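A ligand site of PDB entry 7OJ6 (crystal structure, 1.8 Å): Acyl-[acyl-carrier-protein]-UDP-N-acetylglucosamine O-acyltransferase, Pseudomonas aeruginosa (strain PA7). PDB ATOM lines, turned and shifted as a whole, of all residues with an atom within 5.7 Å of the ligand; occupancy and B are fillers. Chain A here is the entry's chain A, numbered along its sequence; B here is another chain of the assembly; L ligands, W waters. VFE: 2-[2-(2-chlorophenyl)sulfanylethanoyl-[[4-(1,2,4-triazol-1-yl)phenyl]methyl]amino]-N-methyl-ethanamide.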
ATOM      1  N   LEU A 115     -13.876  28.646 -20.547  1.00  0.00           N
ATOM      2  CA  LEU A 115     -13.425  27.240 -20.676  1.00  0.00           C
ATOM      3  C   LEU A 115     -14.159  26.652 -21.845  1.00  0.00           C
ATOM      4  O   LEU A 115     -15.417  26.556 -21.836  1.00  0.00           O
ATOM      5  CB  LEU A 115     -13.743  26.475 -19.384  1.00  0.00           C
ATOM      6  CG  LEU A 115     -13.431  24.941 -19.528  1.00  0.00           C
ATOM      7  CD1 LEU A 115     -12.007  24.631 -19.882  1.00  0.00           C
ATOM      8  CD2 LEU A 115     -13.763  24.364 -18.174  1.00  0.00           C
ATOM      9  N   MET A 117     -14.268  23.346 -24.056  1.00  0.00           N
ATOM     10  CA  MET A 117     -13.840  22.011 -23.786  1.00  0.00           C
ATOM     11  C   MET A 117     -13.718  21.257 -25.112  1.00  0.00           C
ATOM     12  O   MET A 117     -14.032  21.780 -26.180  1.00  0.00           O
ATOM     13  CB  MET A 117     -14.781  21.329 -22.761  1.00  0.00           C
ATOM     14  CG  MET A 117     -14.599  22.020 -21.420  1.00  0.00           C
ATOM     15  SD  MET A 117     -15.739  21.363 -20.156  1.00  0.00           S
ATOM     16  CE  MET A 117     -14.962  19.845 -19.816  1.00  0.00           C
ATOM     17  N   ILE A 133     -18.695  28.404 -19.907  1.00  0.00           N
ATOM     18  CA  ILE A 133     -18.179  27.011 -20.073  1.00  0.00           C
ATOM     19  C   ILE A 133     -18.956  26.454 -21.217  1.00  0.00           C
ATOM     20  O   ILE A 133     -20.186  26.377 -21.154  1.00  0.00           O
ATOM     21  CB  ILE A 133     -18.406  26.206 -18.826  1.00  0.00           C
ATOM     22  CG1 ILE A 133     -17.650  26.812 -17.610  1.00  0.00           C
ATOM     23  CG2 ILE A 133     -17.822  24.803 -19.102  1.00  0.00           C
ATOM     24  CD1 ILE A 133     -17.846  26.159 -16.270  1.00  0.00           C
ATOM     25  N   VAL A 135     -19.066  22.950 -22.864  1.00  0.00           N
ATOM     26  CA  VAL A 135     -18.607  21.612 -22.582  1.00  0.00           C
ATOM     27  C   VAL A 135     -18.365  20.902 -23.934  1.00  0.00           C
ATOM     28  O   VAL A 135     -18.792  21.384 -25.013  1.00  0.00           O
ATOM     29  CB  VAL A 135     -19.623  20.875 -21.660  1.00  0.00           C
ATOM     30  CG1 VAL A 135     -19.175  19.479 -21.261  1.00  0.00           C
ATOM     31  CG2 VAL A 135     -19.761  21.733 -20.374  1.00  0.00           C
ATOM     32  N   ASN A 136     -17.697  19.787 -23.845  1.00  0.00           N
ATOM     33  CA  ASN A 136     -17.334  18.965 -25.021  1.00  0.00           C
ATOM     34  C   ASN A 136     -18.355  18.983 -26.146  1.00  0.00           C
ATOM     35  O   ASN A 136     -19.475  18.609 -25.930  1.00  0.00           O
ATOM     36  CB  ASN A 136     -17.122  17.518 -24.692  1.00  0.00           C
ATOM     37  CG  ASN A 136     -15.933  17.313 -23.741  1.00  0.00           C
ATOM     38  OD1 ASN A 136     -15.884  17.934 -22.657  1.00  0.00           O
ATOM     39  ND2 ASN A 136     -15.205  16.282 -23.993  1.00  0.00           N
ATOM     40  N   ILE A 151     -23.456  28.293 -19.099  1.00  0.00           N
ATOM     41  CA  ILE A 151     -22.906  26.884 -19.155  1.00  0.00           C
ATOM     42  C   ILE A 151     -23.703  26.091 -20.152  1.00  0.00           C
ATOM     43  O   ILE A 151     -24.918  25.993 -20.073  1.00  0.00           O
ATOM     44  CB  ILE A 151     -23.074  26.216 -17.842  1.00  0.00           C
ATOM     45  CG1 ILE A 151     -22.246  26.960 -16.742  1.00  0.00           C
ATOM     46  CG2 ILE A 151     -22.590  24.744 -17.924  1.00  0.00           C
ATOM     47  CD1 ILE A 151     -22.412  26.341 -15.322  1.00  0.00           C
ATOM     48  N   LEU A 152     -23.043  25.672 -21.204  1.00  0.00           N
ATOM     49  CA  LEU A 152     -23.664  24.857 -22.233  1.00  0.00           C
ATOM     50  C   LEU A 152     -23.113  23.408 -22.058  1.00  0.00           C
ATOM     51  O   LEU A 152     -21.914  23.166 -22.336  1.00  0.00           O
ATOM     52  CB  LEU A 152     -23.372  25.422 -23.601  1.00  0.00           C
ATOM     53  CG  LEU A 152     -23.874  26.887 -23.841  1.00  0.00           C
ATOM     54  CD1 LEU A 152     -23.626  27.234 -25.283  1.00  0.00           C
ATOM     55  CD2 LEU A 152     -25.392  26.929 -23.774  1.00  0.00           C
ATOM     56  N   SER A 153     -23.940  22.491 -21.631  1.00  0.00           N
ATOM     57  CA  SER A 153     -23.495  21.171 -21.351  1.00  0.00           C
ATOM     58  C   SER A 153     -23.115  20.415 -22.665  1.00  0.00           C
ATOM     59  O   SER A 153     -23.394  20.867 -23.747  1.00  0.00           O
ATOM     60  CB  SER A 153     -24.524  20.319 -20.559  1.00  0.00           C
ATOM     61  OG  SER A 153     -24.822  20.925 -19.309  1.00  0.00           O
ATOM     62  N   GLY A 154     -22.501  19.255 -22.489  1.00  0.00           N
ATOM     63  CA  GLY A 154     -21.931  18.522 -23.613  1.00  0.00           C
ATOM     64  C   GLY A 154     -22.885  18.326 -24.708  1.00  0.00           C
ATOM     65  O   GLY A 154     -24.019  17.991 -24.539  1.00  0.00           O
ATOM     66  N   TYR A 155     -22.323  18.530 -25.950  1.00  0.00           N
ATOM     67  CA  TYR A 155     -23.134  18.241 -27.106  1.00  0.00           C
ATOM     68  C   TYR A 155     -24.306  19.158 -27.276  1.00  0.00           C
ATOM     69  O   TYR A 155     -25.291  18.833 -27.984  1.00  0.00           O
ATOM     70  CB  TYR A 155     -23.483  16.735 -27.287  1.00  0.00           C
ATOM     71  CG  TYR A 155     -22.296  15.915 -27.612  1.00  0.00           C
ATOM     72  CD1 TYR A 155     -21.345  15.576 -26.635  1.00  0.00           C
ATOM     73  CD2 TYR A 155     -22.158  15.335 -28.903  1.00  0.00           C
ATOM     74  CE1 TYR A 155     -20.211  14.796 -26.940  1.00  0.00           C
ATOM     75  CE2 TYR A 155     -21.062  14.532 -29.181  1.00  0.00           C
ATOM     76  CZ  TYR A 155     -20.081  14.291 -28.190  1.00  0.00           C
ATOM     77  OH  TYR A 155     -18.991  13.470 -28.574  1.00  0.00           O
ATOM     78  N   PHE A 169     -28.282  27.983 -18.628  1.00  0.00           N
ATOM     79  CA  PHE A 169     -27.723  26.621 -18.600  1.00  0.00           C
ATOM     80  C   PHE A 169     -28.500  25.781 -19.639  1.00  0.00           C
ATOM     81  O   PHE A 169     -29.713  25.766 -19.657  1.00  0.00           O
ATOM     82  CB  PHE A 169     -27.994  26.001 -17.203  1.00  0.00           C
ATOM     83  CG  PHE A 169     -27.608  24.547 -17.047  1.00  0.00           C
ATOM     84  CD1 PHE A 169     -26.268  24.152 -16.723  1.00  0.00           C
ATOM     85  CD2 PHE A 169     -28.550  23.562 -17.264  1.00  0.00           C
ATOM     86  CE1 PHE A 169     -25.929  22.824 -16.607  1.00  0.00           C
ATOM     87  CE2 PHE A 169     -28.169  22.167 -17.167  1.00  0.00           C
ATOM     88  CZ  PHE A 169     -26.906  21.806 -16.756  1.00  0.00           C
ATOM     89  N   MET A 172     -27.425  18.356 -21.296  1.00  0.00           N
ATOM     90  CA  MET A 172     -26.606  17.659 -22.318  1.00  0.00           C
ATOM     91  C   MET A 172     -27.434  17.354 -23.484  1.00  0.00           C
ATOM     92  O   MET A 172     -28.556  16.994 -23.367  1.00  0.00           O
ATOM     93  CB  MET A 172     -25.886  16.370 -21.721  1.00  0.00           C
ATOM     94  CG  MET A 172     -26.597  15.311 -21.337  1.00  0.00           C
ATOM     95  SD  MET A 172     -25.457  13.847 -20.913  1.00  0.00           S
ATOM     96  CE  MET A 172     -26.911  12.971 -20.843  1.00  0.00           C
ATOM     97  N   PRO B  72     -10.237  17.312 -14.034  1.00  0.00           N
ATOM     98  CA  PRO B  72     -10.753  18.676 -13.480  1.00  0.00           C
ATOM     99  C   PRO B  72     -11.046  18.713 -11.882  1.00  0.00           C
ATOM    100  O   PRO B  72     -11.312  17.642 -11.304  1.00  0.00           O
ATOM    101  CB  PRO B  72     -12.051  18.924 -14.340  1.00  0.00           C
ATOM    102  CG  PRO B  72     -12.513  17.529 -14.719  1.00  0.00           C
ATOM    103  CD  PRO B  72     -11.254  16.651 -14.896  1.00  0.00           C
ATOM    104  N   HIS B 121     -15.216   9.871 -25.649  1.00  0.00           N
ATOM    105  CA  HIS B 121     -14.679  10.584 -24.567  1.00  0.00           C
ATOM    106  C   HIS B 121     -14.969   9.799 -23.202  1.00  0.00           C
ATOM    107  O   HIS B 121     -16.138   9.413 -22.978  1.00  0.00           O
ATOM    108  CB  HIS B 121     -15.350  11.911 -24.465  1.00  0.00           C
ATOM    109  CG  HIS B 121     -15.018  12.612 -23.190  1.00  0.00           C
ATOM    110  ND1 HIS B 121     -13.824  13.195 -22.965  1.00  0.00           N
ATOM    111  CD2 HIS B 121     -15.716  12.787 -22.027  1.00  0.00           C
ATOM    112  CE1 HIS B 121     -13.781  13.787 -21.785  1.00  0.00           C
ATOM    113  NE2 HIS B 121     -14.926  13.528 -21.174  1.00  0.00           N
ATOM    114  N   HIS B 124     -13.175  11.529 -16.296  1.00  0.00           N
ATOM    115  CA  HIS B 124     -12.503  11.229 -15.086  1.00  0.00           C
ATOM    116  C   HIS B 124     -13.308  10.214 -14.145  1.00  0.00           C
ATOM    117  O   HIS B 124     -14.514  10.342 -13.945  1.00  0.00           O
ATOM    118  CB  HIS B 124     -12.140  12.448 -14.203  1.00  0.00           C
ATOM    119  CG  HIS B 124     -13.289  13.193 -13.666  1.00  0.00           C
ATOM    120  ND1 HIS B 124     -14.075  13.997 -14.451  1.00  0.00           N
ATOM    121  CD2 HIS B 124     -13.791  13.265 -12.417  1.00  0.00           C
ATOM    122  CE1 HIS B 124     -15.022  14.555 -13.710  1.00  0.00           C
ATOM    123  NE2 HIS B 124     -14.860  14.140 -12.488  1.00  0.00           N
ATOM    124  N   ALA B 139     -19.932   9.708 -25.149  1.00  0.00           N
ATOM    125  CA  ALA B 139     -19.218  10.536 -24.116  1.00  0.00           C
ATOM    126  C   ALA B 139     -19.745  10.110 -22.741  1.00  0.00           C
ATOM    127  O   ALA B 139     -20.950  10.154 -22.519  1.00  0.00           O
ATOM    128  CB  ALA B 139     -19.479  11.969 -24.424  1.00  0.00           C
ATOM    129  N   LEU B 140     -18.794   9.758 -21.877  1.00  0.00           N
ATOM    130  CA  LEU B 140     -19.068   9.482 -20.489  1.00  0.00           C
ATOM    131  C   LEU B 140     -18.602  10.681 -19.706  1.00  0.00           C
ATOM    132  O   LEU B 140     -17.408  11.022 -19.694  1.00  0.00           O
ATOM    133  CB  LEU B 140     -18.281   8.226 -20.034  1.00  0.00           C
ATOM    134  CG  LEU B 140     -18.396   7.014 -20.954  1.00  0.00           C
ATOM    135  CD1 LEU B 140     -17.648   5.842 -20.256  1.00  0.00           C
ATOM    136  CD2 LEU B 140     -19.784   6.593 -21.359  1.00  0.00           C
ATOM    137  N   ALA B 141     -19.509  11.381 -19.108  1.00  0.00           N
ATOM    138  CA  ALA B 141     -19.207  12.639 -18.452  1.00  0.00           C
ATOM    139  C   ALA B 141     -18.218  12.583 -17.276  1.00  0.00           C
ATOM    140  O   ALA B 141     -17.310  13.420 -17.094  1.00  0.00           O
ATOM    141  CB  ALA B 141     -20.412  13.377 -17.971  1.00  0.00           C
ATOM    142  N   LEU B 157     -24.601   9.862 -25.019  1.00  0.00           N
ATOM    143  CA  LEU B 157     -24.134  10.681 -23.980  1.00  0.00           C
ATOM    144  C   LEU B 157     -24.607  10.134 -22.572  1.00  0.00           C
ATOM    145  O   LEU B 157     -25.788   9.788 -22.470  1.00  0.00           O
ATOM    146  CB  LEU B 157     -24.775  12.070 -24.141  1.00  0.00           C
ATOM    147  CG  LEU B 157     -24.670  12.713 -25.617  1.00  0.00           C
ATOM    148  CD1 LEU B 157     -25.337  14.031 -25.517  1.00  0.00           C
ATOM    149  CD2 LEU B 157     -23.256  12.648 -25.990  1.00  0.00           C
ATOM    150  N   VAL B 158     -23.698  10.081 -21.602  1.00  0.00           N
ATOM    151  CA  VAL B 158     -23.962   9.512 -20.346  1.00  0.00           C
ATOM    152  C   VAL B 158     -23.641  10.510 -19.238  1.00  0.00           C
ATOM    153  O   VAL B 158     -22.479  10.927 -19.102  1.00  0.00           O
ATOM    154  CB  VAL B 158     -23.179   8.245 -20.141  1.00  0.00           C
ATOM    155  CG1 VAL B 158     -23.666   7.584 -18.864  1.00  0.00           C
ATOM    156  CG2 VAL B 158     -23.421   7.184 -21.307  1.00  0.00           C
ATOM    157  N   HIS B 159     -24.662  10.865 -18.469  1.00  0.00           N
ATOM    158  CA  HIS B 159     -24.619  11.755 -17.325  1.00  0.00           C
ATOM    159  C   HIS B 159     -23.642  11.163 -16.274  1.00  0.00           C
ATOM    160  O   HIS B 159     -23.506   9.911 -16.161  1.00  0.00           O
ATOM    161  CB  HIS B 159     -26.016  11.917 -16.754  1.00  0.00           C
ATOM    162  CG  HIS B 159     -26.188  12.942 -15.723  1.00  0.00           C
ATOM    163  ND1 HIS B 159     -25.737  12.835 -14.400  1.00  0.00           N
ATOM    164  CD2 HIS B 159     -26.888  14.118 -15.758  1.00  0.00           C
ATOM    165  CE1 HIS B 159     -25.996  13.936 -13.732  1.00  0.00           C
ATOM    166  NE2 HIS B 159     -26.785  14.666 -14.492  1.00  0.00           N
ATOM    167  N   GLN B 160     -23.054  12.043 -15.490  1.00  0.00           N
ATOM    168  CA  GLN B 160     -22.095  11.679 -14.446  1.00  0.00           C
ATOM    169  C   GLN B 160     -22.869  10.681 -13.481  1.00  0.00           C
ATOM    170  O   GLN B 160     -24.028  10.877 -13.180  1.00  0.00           O
ATOM    171  CB  GLN B 160     -21.667  12.847 -13.566  1.00  0.00           C
ATOM    172  CG  GLN B 160     -20.626  13.763 -14.292  1.00  0.00           C
ATOM    173  CD  GLN B 160     -19.966  14.593 -13.263  1.00  0.00           C
ATOM    174  OE1 GLN B 160     -20.564  15.493 -12.628  1.00  0.00           O
ATOM    175  NE2 GLN B 160     -18.747  14.281 -13.012  1.00  0.00           N
HETATM  176  C25 VFE L   1     -18.303  16.301 -19.980  1.00  0.00           C
HETATM  177  C26 VFE L   1     -17.986  15.761 -21.200  1.00  0.00           C
HETATM  178  C9  VFE L   1     -20.019  21.965 -15.993  1.00  0.00           C
HETATM  179  C13 VFE L   1     -19.207  20.119 -17.240  1.00  0.00           C
HETATM  180  C10 VFE L   1     -18.720  22.308 -15.673  1.00  0.00           C
HETATM  181  C12 VFE L   1     -17.929  20.456 -16.928  1.00  0.00           C
HETATM  182  C24 VFE L   1     -19.630  16.399 -19.641  1.00  0.00           C
HETATM  183  C27 VFE L   1     -18.946  15.306 -22.044  1.00  0.00           C
HETATM  184  C17 VFE L   1     -14.801  22.907 -15.013  1.00  0.00           C
HETATM  185  C15 VFE L   1     -15.150  21.293 -16.176  1.00  0.00           C
HETATM  186  C8  VFE L   1     -20.275  20.855 -16.797  1.00  0.00           C
HETATM  187  C11 VFE L   1     -17.677  21.560 -16.147  1.00  0.00           C
HETATM  188  C23 VFE L   1     -20.653  16.027 -20.475  1.00  0.00           C
HETATM  189  C28 VFE L   1     -20.263  15.395 -21.701  1.00  0.00           C
HETATM  190  C3  VFE L   1     -20.515  17.819 -15.641  1.00  0.00           C
HETATM  191  C19 VFE L   1     -22.025  18.352 -18.496  1.00  0.00           C
HETATM  192  C1  VFE L   1     -18.805  18.091 -13.863  1.00  0.00           C
HETATM  193  C7  VFE L   1     -21.640  20.453 -17.200  1.00  0.00           C
HETATM  194  C5  VFE L   1     -21.872  18.302 -15.986  1.00  0.00           C
HETATM  195  C21 VFE L   1     -22.310  16.841 -18.485  1.00  0.00           C
HETATM  196  N16 VFE L   1     -14.098  21.910 -15.670  1.00  0.00           N
HETATM  197  N18 VFE L   1     -16.139  22.942 -15.068  1.00  0.00           N
HETATM  198  N14 VFE L   1     -16.347  21.882 -15.827  1.00  0.00           N
HETATM  199  N2  VFE L   1     -20.061  18.387 -14.472  1.00  0.00           N
HETATM  200  N6  VFE L   1     -21.774  18.973 -17.287  1.00  0.00           N
HETATM  201  O4  VFE L   1     -19.850  17.002 -16.281  1.00  0.00           O
HETATM  202  O20 VFE L   1     -22.117  18.929 -19.566  1.00  0.00           O
HETATM  203  S22 VFE L   1     -22.376  16.110 -20.165  1.00  0.00           S
HETATM  204 CL   VFE L   1     -21.528  14.856 -22.713  1.00  0.00          CL
HETATM  205  O   HOH W   1     -16.324  20.574 -12.583  1.00  0.00           O
HETATM  206  O   HOH W   2     -17.201  24.409 -13.197  1.00  0.00           O
HETATM  207  O   HOH W   3     -11.446  21.684 -15.830  1.00  0.00           O
HETATM  208  O   HOH W   4     -25.189  15.338 -18.161  1.00  0.00           O
HETATM  209  O   HOH W   5     -23.494  14.878 -15.870  1.00  0.00           O
HETATM  210  O   HOH W   6     -21.235  20.635 -12.781  1.00  0.00           O
HETATM  211  O   HOH W   7     -15.432  17.944 -16.773  1.00  0.00           O
HETATM  212  O   HOH W   8     -25.020  18.821 -17.524  1.00  0.00           O
HETATM  213  O   HOH W   9     -17.350  15.969 -16.221  1.00  0.00           O
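The backbone NH (N) of Gly 154 sits at hydrogen-bond distance from an oxygen (O20) of the ligand (3.0 Å).
The side-chain hydroxyl (OG) of Ser 153 sits close to an oxygen (O20) of the ligand (3.4 Å).
The side-chain amide oxygen of Gln 160 of chain B sits close to a nitrogen (N2) of the ligand (3.5 Å).
N of Leu 152 sits at hydrogen-bond distance from O of Ile 133 (2.9 Å).
The backbone NH (N) of Val 135 sits at hydrogen-bond distance from the backbone carbonyl oxygen (O) of Leu 152 (2.9 Å).
The backbone carbonyl oxygen of His 121 of chain B lies within hydrogen-bond range of the backbone NH of Leu 140 of chain B (2.9 Å).
The backbone carbonyl oxygen of Ala 139 of chain B is in hydrogen-bond range of the backbone NH of Val 158 of chain B (2.9 Å).
The backbone carbonyl oxygen of Val 158 of chain B sits at hydrogen-bond distance from the backbone NH of Ala 141 of chain B, 3.0 Å away.
The backbone NH of Tyr 155 is in hydrogen-bond range of the backbone carbonyl oxygen of Asn 136 (2.8 Å).
Merely in contact with the ligand: Asn 136, Val 135, Leu 115, Ala 141 of chain B, His 121 of chain B, Ile 133, Met 172, Pro 72 of chain B, Met 117, Ala 139 of chain B and Tyr 155.
Hydrophobic or aromatic side chains that line the ligand: Leu 115, Met 117, Ile 133, Val 135, Tyr 155, Met 172, Pro 72 of chain B, His 121 of chain B, Ala 139 of chain B and Ala 141 of chain B.
14 residues have an atom within 4 Å of the ligand: Leu 115, Met 117, Ile 133, Val 135, Asn 136, Ser 153, Gly 154, Tyr 155, Met 172, Pro 72 of chain B, His 121 of chain B, Ala 139 of chain B, Ala 141 of chain B and Gln 160 of chain B.
The nearest printed residue that does not touch the ligand is Ile 151 (4.2 Å).
Water W9 bridges O of Ala 141 of chain B (2.7 Å) and O4 of the ligand (2.7 Å).
Water W4 bridges the side-chain sulfur of Met 172 and a sulfur (S22) of the ligand.
Water W5 lies within hydrogen-bond range of N of Gln 160 of chain B (2.9 Å) and ND1 of His 159 of chain B (3.4 Å).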
